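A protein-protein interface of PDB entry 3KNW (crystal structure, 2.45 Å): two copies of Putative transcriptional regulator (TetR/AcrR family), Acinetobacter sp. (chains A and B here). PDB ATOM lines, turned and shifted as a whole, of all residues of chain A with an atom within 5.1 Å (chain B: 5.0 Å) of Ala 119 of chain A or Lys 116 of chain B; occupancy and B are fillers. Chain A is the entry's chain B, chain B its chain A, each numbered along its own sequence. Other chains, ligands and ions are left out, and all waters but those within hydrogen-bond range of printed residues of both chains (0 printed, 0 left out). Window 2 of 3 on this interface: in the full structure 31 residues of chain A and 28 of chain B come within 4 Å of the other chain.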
ATOM      1  N   ILE A 114       9.065  21.992 -16.507  1.00  0.00           N
ATOM      2  CA  ILE A 114       8.265  22.970 -15.745  1.00  0.00           C
ATOM      3  C   ILE A 114       9.170  23.626 -14.678  1.00  0.00           C
ATOM      4  O   ILE A 114       9.119  24.832 -14.490  1.00  0.00           O
ATOM      5  CB  ILE A 114       6.980  22.381 -15.138  1.00  0.00           C
ATOM      6  CG1 ILE A 114       6.019  21.979 -16.233  1.00  0.00           C
ATOM      7  CG2 ILE A 114       6.226  23.417 -14.299  1.00  0.00           C
ATOM      8  CD1 ILE A 114       4.628  21.734 -15.712  1.00  0.00           C
ATOM      9  N   VAL A 115      10.033  22.839 -14.038  1.00  0.00           N
ATOM     10  CA  VAL A 115      10.999  23.377 -13.070  1.00  0.00           C
ATOM     11  C   VAL A 115      11.924  24.416 -13.669  1.00  0.00           C
ATOM     12  O   VAL A 115      12.018  25.551 -13.158  1.00  0.00           O
ATOM     13  CB  VAL A 115      11.846  22.258 -12.399  1.00  0.00           C
ATOM     14  CG1 VAL A 115      12.885  22.867 -11.449  1.00  0.00           C
ATOM     15  CG2 VAL A 115      10.942  21.246 -11.655  1.00  0.00           C
ATOM     16  N   LYS A 116      12.597  24.050 -14.763  1.00  0.00           N
ATOM     17  CA  LYS A 116      13.529  24.957 -15.417  1.00  0.00           C
ATOM     18  C   LYS A 116      12.834  26.192 -15.943  1.00  0.00           C
ATOM     19  O   LYS A 116      13.383  27.283 -15.910  1.00  0.00           O
ATOM     20  CB  LYS A 116      14.282  24.258 -16.564  1.00  0.00           C
ATOM     21  CG  LYS A 116      15.229  23.147 -16.090  1.00  0.00           C
ATOM     22  CD  LYS A 116      16.468  23.013 -16.982  1.00  0.00           C
ATOM     23  CE  LYS A 116      17.688  22.467 -16.225  1.00  0.00           C
ATOM     24  NZ  LYS A 116      18.755  23.523 -16.078  1.00  0.00           N
ATOM     25  N   MET A 117      11.626  26.025 -16.443  1.00  0.00           N
ATOM     26  CA  MET A 117      10.901  27.165 -16.953  1.00  0.00           C
ATOM     27  C   MET A 117      10.402  28.023 -15.768  1.00  0.00           C
ATOM     28  O   MET A 117      10.546  29.261 -15.787  1.00  0.00           O
ATOM     29  CB  MET A 117       9.742  26.726 -17.879  1.00  0.00           C
ATOM     30  CG  MET A 117      10.136  26.063 -19.225  1.00  0.00           C
ATOM     31  SD  MET A 117      11.343  27.003 -20.376  1.00  0.00           S
ATOM     32  CE  MET A 117      13.046  26.195 -19.991  1.00  0.00           C
ATOM     33  N   ALA A 118       9.829  27.379 -14.746  1.00  0.00           N
ATOM     34  CA  ALA A 118       9.466  28.101 -13.527  1.00  0.00           C
ATOM     35  C   ALA A 118      10.718  28.803 -12.937  1.00  0.00           C
ATOM     36  O   ALA A 118      10.662  29.963 -12.526  1.00  0.00           O
ATOM     37  CB  ALA A 118       8.795  27.167 -12.496  1.00  0.00           C
ATOM     38  N   ALA A 119      11.858  28.119 -12.956  1.00  0.00           N
ATOM     39  CA  ALA A 119      13.120  28.724 -12.481  1.00  0.00           C
ATOM     40  C   ALA A 119      13.601  29.950 -13.271  1.00  0.00           C
ATOM     41  O   ALA A 119      14.425  30.680 -12.784  1.00  0.00           O
ATOM     42  CB  ALA A 119      14.240  27.673 -12.399  1.00  0.00           C
ATOM     43  N   GLU A 120      13.072  30.187 -14.469  1.00  0.00           N
ATOM     44  CA  GLU A 120      13.539  31.276 -15.332  1.00  0.00           C
ATOM     45  C   GLU A 120      12.449  32.270 -15.716  1.00  0.00           C
ATOM     46  O   GLU A 120      12.671  33.131 -16.579  1.00  0.00           O
ATOM     47  CB  GLU A 120      14.037  30.691 -16.647  1.00  0.00           C
ATOM     48  CG  GLU A 120      15.228  29.747 -16.588  1.00  0.00           C
ATOM     49  CD  GLU A 120      15.589  29.236 -18.008  1.00  0.00           C
ATOM     50  OE1 GLU A 120      14.698  29.299 -18.908  1.00  0.00           O
ATOM     51  OE2 GLU A 120      16.755  28.804 -18.231  1.00  0.00           O
ATOM     52  N   VAL A 121      11.279  32.157 -15.093  1.00  0.00           N
ATOM     53  CA  VAL A 121      10.049  32.856 -15.518  1.00  0.00           C
ATOM     54  C   VAL A 121      10.193  34.368 -15.762  1.00  0.00           C
ATOM     55  O   VAL A 121       9.483  34.955 -16.591  1.00  0.00           O
ATOM     56  CB  VAL A 121       8.963  32.677 -14.446  1.00  0.00           C
ATOM     57  CG1 VAL A 121       7.695  33.475 -14.819  1.00  0.00           C
ATOM     58  CG2 VAL A 121       8.638  31.180 -14.250  1.00  0.00           C
ATOM     59  N   VAL B  27      20.976  35.086  -5.201  1.00  0.00           N
ATOM     60  CA  VAL B  27      20.660  33.712  -5.586  1.00  0.00           C
ATOM     61  C   VAL B  27      19.161  33.462  -5.796  1.00  0.00           C
ATOM     62  O   VAL B  27      18.809  32.640  -6.610  1.00  0.00           O
ATOM     63  CB  VAL B  27      21.244  32.670  -4.580  1.00  0.00           C
ATOM     64  CG1 VAL B  27      20.754  31.242  -4.906  1.00  0.00           C
ATOM     65  CG2 VAL B  27      22.760  32.711  -4.582  1.00  0.00           C
ATOM     66  N   LEU B  28      18.276  34.146  -5.085  1.00  0.00           N
ATOM     67  CA  LEU B  28      16.841  34.036  -5.386  1.00  0.00           C
ATOM     68  C   LEU B  28      16.508  34.480  -6.811  1.00  0.00           C
ATOM     69  O   LEU B  28      15.615  33.914  -7.437  1.00  0.00           O
ATOM     70  CB  LEU B  28      16.009  34.891  -4.441  1.00  0.00           C
ATOM     71  CG  LEU B  28      15.950  34.514  -2.962  1.00  0.00           C
ATOM     72  CD1 LEU B  28      16.186  35.767  -2.074  1.00  0.00           C
ATOM     73  CD2 LEU B  28      14.631  33.855  -2.635  1.00  0.00           C
ATOM     74  N   ARG B  29      17.202  35.515  -7.285  1.00  0.00           N
ATOM     75  CA  ARG B  29      17.021  36.059  -8.625  1.00  0.00           C
ATOM     76  C   ARG B  29      17.683  35.199  -9.685  1.00  0.00           C
ATOM     77  O   ARG B  29      17.073  34.927 -10.711  1.00  0.00           O
ATOM     78  CB  ARG B  29      17.604  37.483  -8.747  1.00  0.00           C
ATOM     79  CG  ARG B  29      16.698  38.632  -8.249  1.00  0.00           C
ATOM     80  CD  ARG B  29      17.204  39.259  -6.932  1.00  0.00           C
ATOM     81  NE  ARG B  29      16.733  40.640  -6.714  1.00  0.00           N
ATOM     82  CZ  ARG B  29      17.344  41.557  -5.943  1.00  0.00           C
ATOM     83  NH1 ARG B  29      18.483  41.289  -5.302  1.00  0.00           N
ATOM     84  NH2 ARG B  29      16.817  42.773  -5.827  1.00  0.00           N
ATOM     85  N   LYS B  30      18.926  34.789  -9.456  1.00  0.00           N
ATOM     86  CA  LYS B  30      19.759  34.273 -10.545  1.00  0.00           C
ATOM     87  C   LYS B  30      20.377  32.891 -10.351  1.00  0.00           C
ATOM     88  O   LYS B  30      21.056  32.377 -11.239  1.00  0.00           O
ATOM     89  CB  LYS B  30      20.864  35.289 -10.858  1.00  0.00           C
ATOM     90  CG  LYS B  30      20.316  36.642 -11.369  1.00  0.00           C
ATOM     91  CD  LYS B  30      21.438  37.648 -11.747  1.00  0.00           C
ATOM     92  CE  LYS B  30      20.882  39.076 -11.983  1.00  0.00           C
ATOM     93  NZ  LYS B  30      19.673  39.085 -12.886  1.00  0.00           N
ATOM     94  N   GLY B  31      20.151  32.267  -9.212  1.00  0.00           N
ATOM     95  CA  GLY B  31      20.775  30.987  -8.963  1.00  0.00           C
ATOM     96  C   GLY B  31      22.212  31.132  -8.504  1.00  0.00           C
ATOM     97  O   GLY B  31      22.706  32.263  -8.198  1.00  0.00           O
ATOM     98  N   CYS B 112      11.231  29.445  -3.872  1.00  0.00           N
ATOM     99  CA  CYS B 112      12.065  29.771  -5.044  1.00  0.00           C
ATOM    100  C   CYS B 112      13.461  29.147  -4.906  1.00  0.00           C
ATOM    101  O   CYS B 112      13.984  28.580  -5.856  1.00  0.00           O
ATOM    102  CB  CYS B 112      12.167  31.303  -5.257  1.00  0.00           C
ATOM    103  SG  CYS B 112      12.676  31.832  -6.944  1.00  0.00           S
ATOM    104  N   LEU B 113      14.054  29.225  -3.716  1.00  0.00           N
ATOM    105  CA  LEU B 113      15.380  28.646  -3.511  1.00  0.00           C
ATOM    106  C   LEU B 113      15.381  27.171  -3.831  1.00  0.00           C
ATOM    107  O   LEU B 113      16.317  26.719  -4.438  1.00  0.00           O
ATOM    108  CB  LEU B 113      15.962  28.899  -2.098  1.00  0.00           C
ATOM    109  CG  LEU B 113      17.380  28.288  -1.830  1.00  0.00           C
ATOM    110  CD1 LEU B 113      18.490  29.194  -2.364  1.00  0.00           C
ATOM    111  CD2 LEU B 113      17.695  27.943  -0.339  1.00  0.00           C
ATOM    112  N   ILE B 114      14.361  26.407  -3.453  1.00  0.00           N
ATOM    113  CA  ILE B 114      14.370  24.977  -3.797  1.00  0.00           C
ATOM    114  C   ILE B 114      14.120  24.768  -5.278  1.00  0.00           C
ATOM    115  O   ILE B 114      14.627  23.811  -5.844  1.00  0.00           O
ATOM    116  CB  ILE B 114      13.378  24.117  -2.983  1.00  0.00           C
ATOM    117  CG1 ILE B 114      13.938  23.804  -1.614  1.00  0.00           C
ATOM    118  CG2 ILE B 114      13.158  22.784  -3.623  1.00  0.00           C
ATOM    119  CD1 ILE B 114      12.903  23.192  -0.702  1.00  0.00           C
ATOM    120  N   VAL B 115      13.347  25.651  -5.897  1.00  0.00           N
ATOM    121  CA  VAL B 115      13.029  25.542  -7.312  1.00  0.00           C
ATOM    122  C   VAL B 115      14.255  25.878  -8.127  1.00  0.00           C
ATOM    123  O   VAL B 115      14.633  25.144  -9.063  1.00  0.00           O
ATOM    124  CB  VAL B 115      11.927  26.514  -7.716  1.00  0.00           C
ATOM    125  CG1 VAL B 115      11.972  26.799  -9.240  1.00  0.00           C
ATOM    126  CG2 VAL B 115      10.556  25.995  -7.262  1.00  0.00           C
ATOM    127  N   LYS B 116      14.852  27.027  -7.791  1.00  0.00           N
ATOM    128  CA  LYS B 116      16.139  27.422  -8.370  1.00  0.00           C
ATOM    129  C   LYS B 116      17.132  26.291  -8.214  1.00  0.00           C
ATOM    130  O   LYS B 116      17.552  25.704  -9.189  1.00  0.00           O
ATOM    131  CB  LYS B 116      16.661  28.678  -7.717  1.00  0.00           C
ATOM    132  CG  LYS B 116      16.001  29.988  -8.218  1.00  0.00           C
ATOM    133  CD  LYS B 116      16.335  30.281  -9.687  1.00  0.00           C
ATOM    134  CE  LYS B 116      15.876  31.649 -10.136  1.00  0.00           C
ATOM    135  NZ  LYS B 116      16.735  32.079 -11.322  1.00  0.00           N
ATOM    136  N   MET B 117      17.453  25.904  -6.994  1.00  0.00           N
ATOM    137  CA  MET B 117      18.544  24.945  -6.806  1.00  0.00           C
ATOM    138  C   MET B 117      18.248  23.585  -7.444  1.00  0.00           C
ATOM    139  O   MET B 117      19.171  22.936  -7.964  1.00  0.00           O
ATOM    140  CB  MET B 117      18.877  24.778  -5.334  1.00  0.00           C
ATOM    141  CG  MET B 117      19.212  26.081  -4.620  1.00  0.00           C
ATOM    142  SD  MET B 117      20.826  26.722  -5.285  1.00  0.00           S
ATOM    143  CE  MET B 117      21.851  25.548  -4.207  1.00  0.00           C
ATOM    144  N   ALA B 118      16.983  23.141  -7.411  1.00  0.00           N
ATOM    145  CA  ALA B 118      16.564  21.893  -8.108  1.00  0.00           C
ATOM    146  C   ALA B 118      16.881  22.013  -9.603  1.00  0.00           C
ATOM    147  O   ALA B 118      17.463  21.119 -10.210  1.00  0.00           O
ATOM    148  CB  ALA B 118      15.034  21.611  -7.908  1.00  0.00           C
ATOM    149  N   ALA B 119      16.500  23.154 -10.171  1.00  0.00           N
ATOM    150  CA  ALA B 119      16.770  23.496 -11.553  1.00  0.00           C
ATOM    151  C   ALA B 119      18.222  23.267 -11.954  1.00  0.00           C
ATOM    152  O   ALA B 119      18.492  22.625 -12.984  1.00  0.00           O
ATOM    153  CB  ALA B 119      16.392  24.950 -11.804  1.00  0.00           C
ATOM    154  N   GLU B 120      19.151  23.788 -11.149  1.00  0.00           N
ATOM    155  CA  GLU B 120      20.552  23.714 -11.474  1.00  0.00           C
ATOM    156  C   GLU B 120      21.255  22.601 -10.734  1.00  0.00           C
ATOM    157  O   GLU B 120      22.468  22.646 -10.541  1.00  0.00           O
ATOM    158  CB  GLU B 120      21.229  25.057 -11.136  1.00  0.00           C
ATOM    159  CG  GLU B 120      21.221  25.454  -9.652  1.00  0.00           C
ATOM    160  CD  GLU B 120      22.121  26.640  -9.401  1.00  0.00           C
ATOM    161  OE1 GLU B 120      23.301  26.438  -8.972  1.00  0.00           O
ATOM    162  OE2 GLU B 120      21.640  27.767  -9.652  1.00  0.00           O
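Val 115 of chain B touches Val 115 of chain A. Val 115 of chain A touches Ala 119 of chain B. CA of Ala 119 of chain A touches CG1 of Val 115 of chain B, at 3.9 Å. Ala 119 of chain B touches Ala 119 of chain A (CB to CB, 3.5 Å).
Ala 119 of chain A touches just these residues of chain B: Val 115 (3.9 Å), Lys 116 (3.1 Å) and Ala 119 (3.5 Å). Printed residues of chain A within 4 Å of Lys 116 of chain B: Ala 119 (3.1 Å). Of the printed residues of chain A, Ala 119 of chain B touches Val 115 (3.8 Å), Lys 116 (3.2 Å) and Ala 119 (3.5 Å). Printed residues of chain A within 4 Å of Val 115 of chain B: Val 115 (3.7 Å) and Ala 119 (3.9 Å). Of the printed residues of chain B, Lys 116 of chain A touches Ala 119 (3.2 Å). Of the printed residues of chain B, Val 115 of chain A touches Val 115 and Ala 119. The nearest printed residue of chain B that does not touch Ala 119 of chain A is Arg 29 of chain B (5.4 Å).
Val 115 of chain A touches its own counterpart, Val 115 of chain B. Val 115 of chain A touches Ala 119 of chain B, and with the chains exchanged Ala 119 of chain A touches Val 115 of chain B. Lys 116 of chain A touches Ala 119 of chain B, and with the chains exchanged Ala 119 of chain A touches Lys 116 of chain B. Ala 119 of chain A touches its own counterpart, Ala 119 of chain B. 7 positions are printed for both chains. Of the 6 pairs that touch across the chains among the printed residues, 6 have their exchanged pair printed and touching as well.
Of the 8 printed residues of chain A, 3 touch a printed residue of chain B. Hydrophobic or aromatic side chains of chain A that line the printed part of chain B: Val 115 and Ala 119. Of the 14 printed residues of chain B, 3 touch a printed residue of chain A. Hydrophobic or aromatic side chains of chain B that line the printed part of chain A: Val 115 and Ala 119. Among the printed residues, 6 pairs touch across the chains.
The side-chain amino group (NZ) of Lys 116 of chain B is in hydrogen-bond range of the backbone carbonyl oxygen (O) of Ala 119 of chain A (3.1 Å). The backbone carbonyl oxygen of Ala 119 of chain B sits at hydrogen-bond distance from the side-chain amino group of Lys 116 of chain A (3.2 Å).
The backbone carbonyl oxygen of Arg 29 of chain B sits at hydrogen-bond distance from the side-chain amino group of Lys 116 of chain B.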
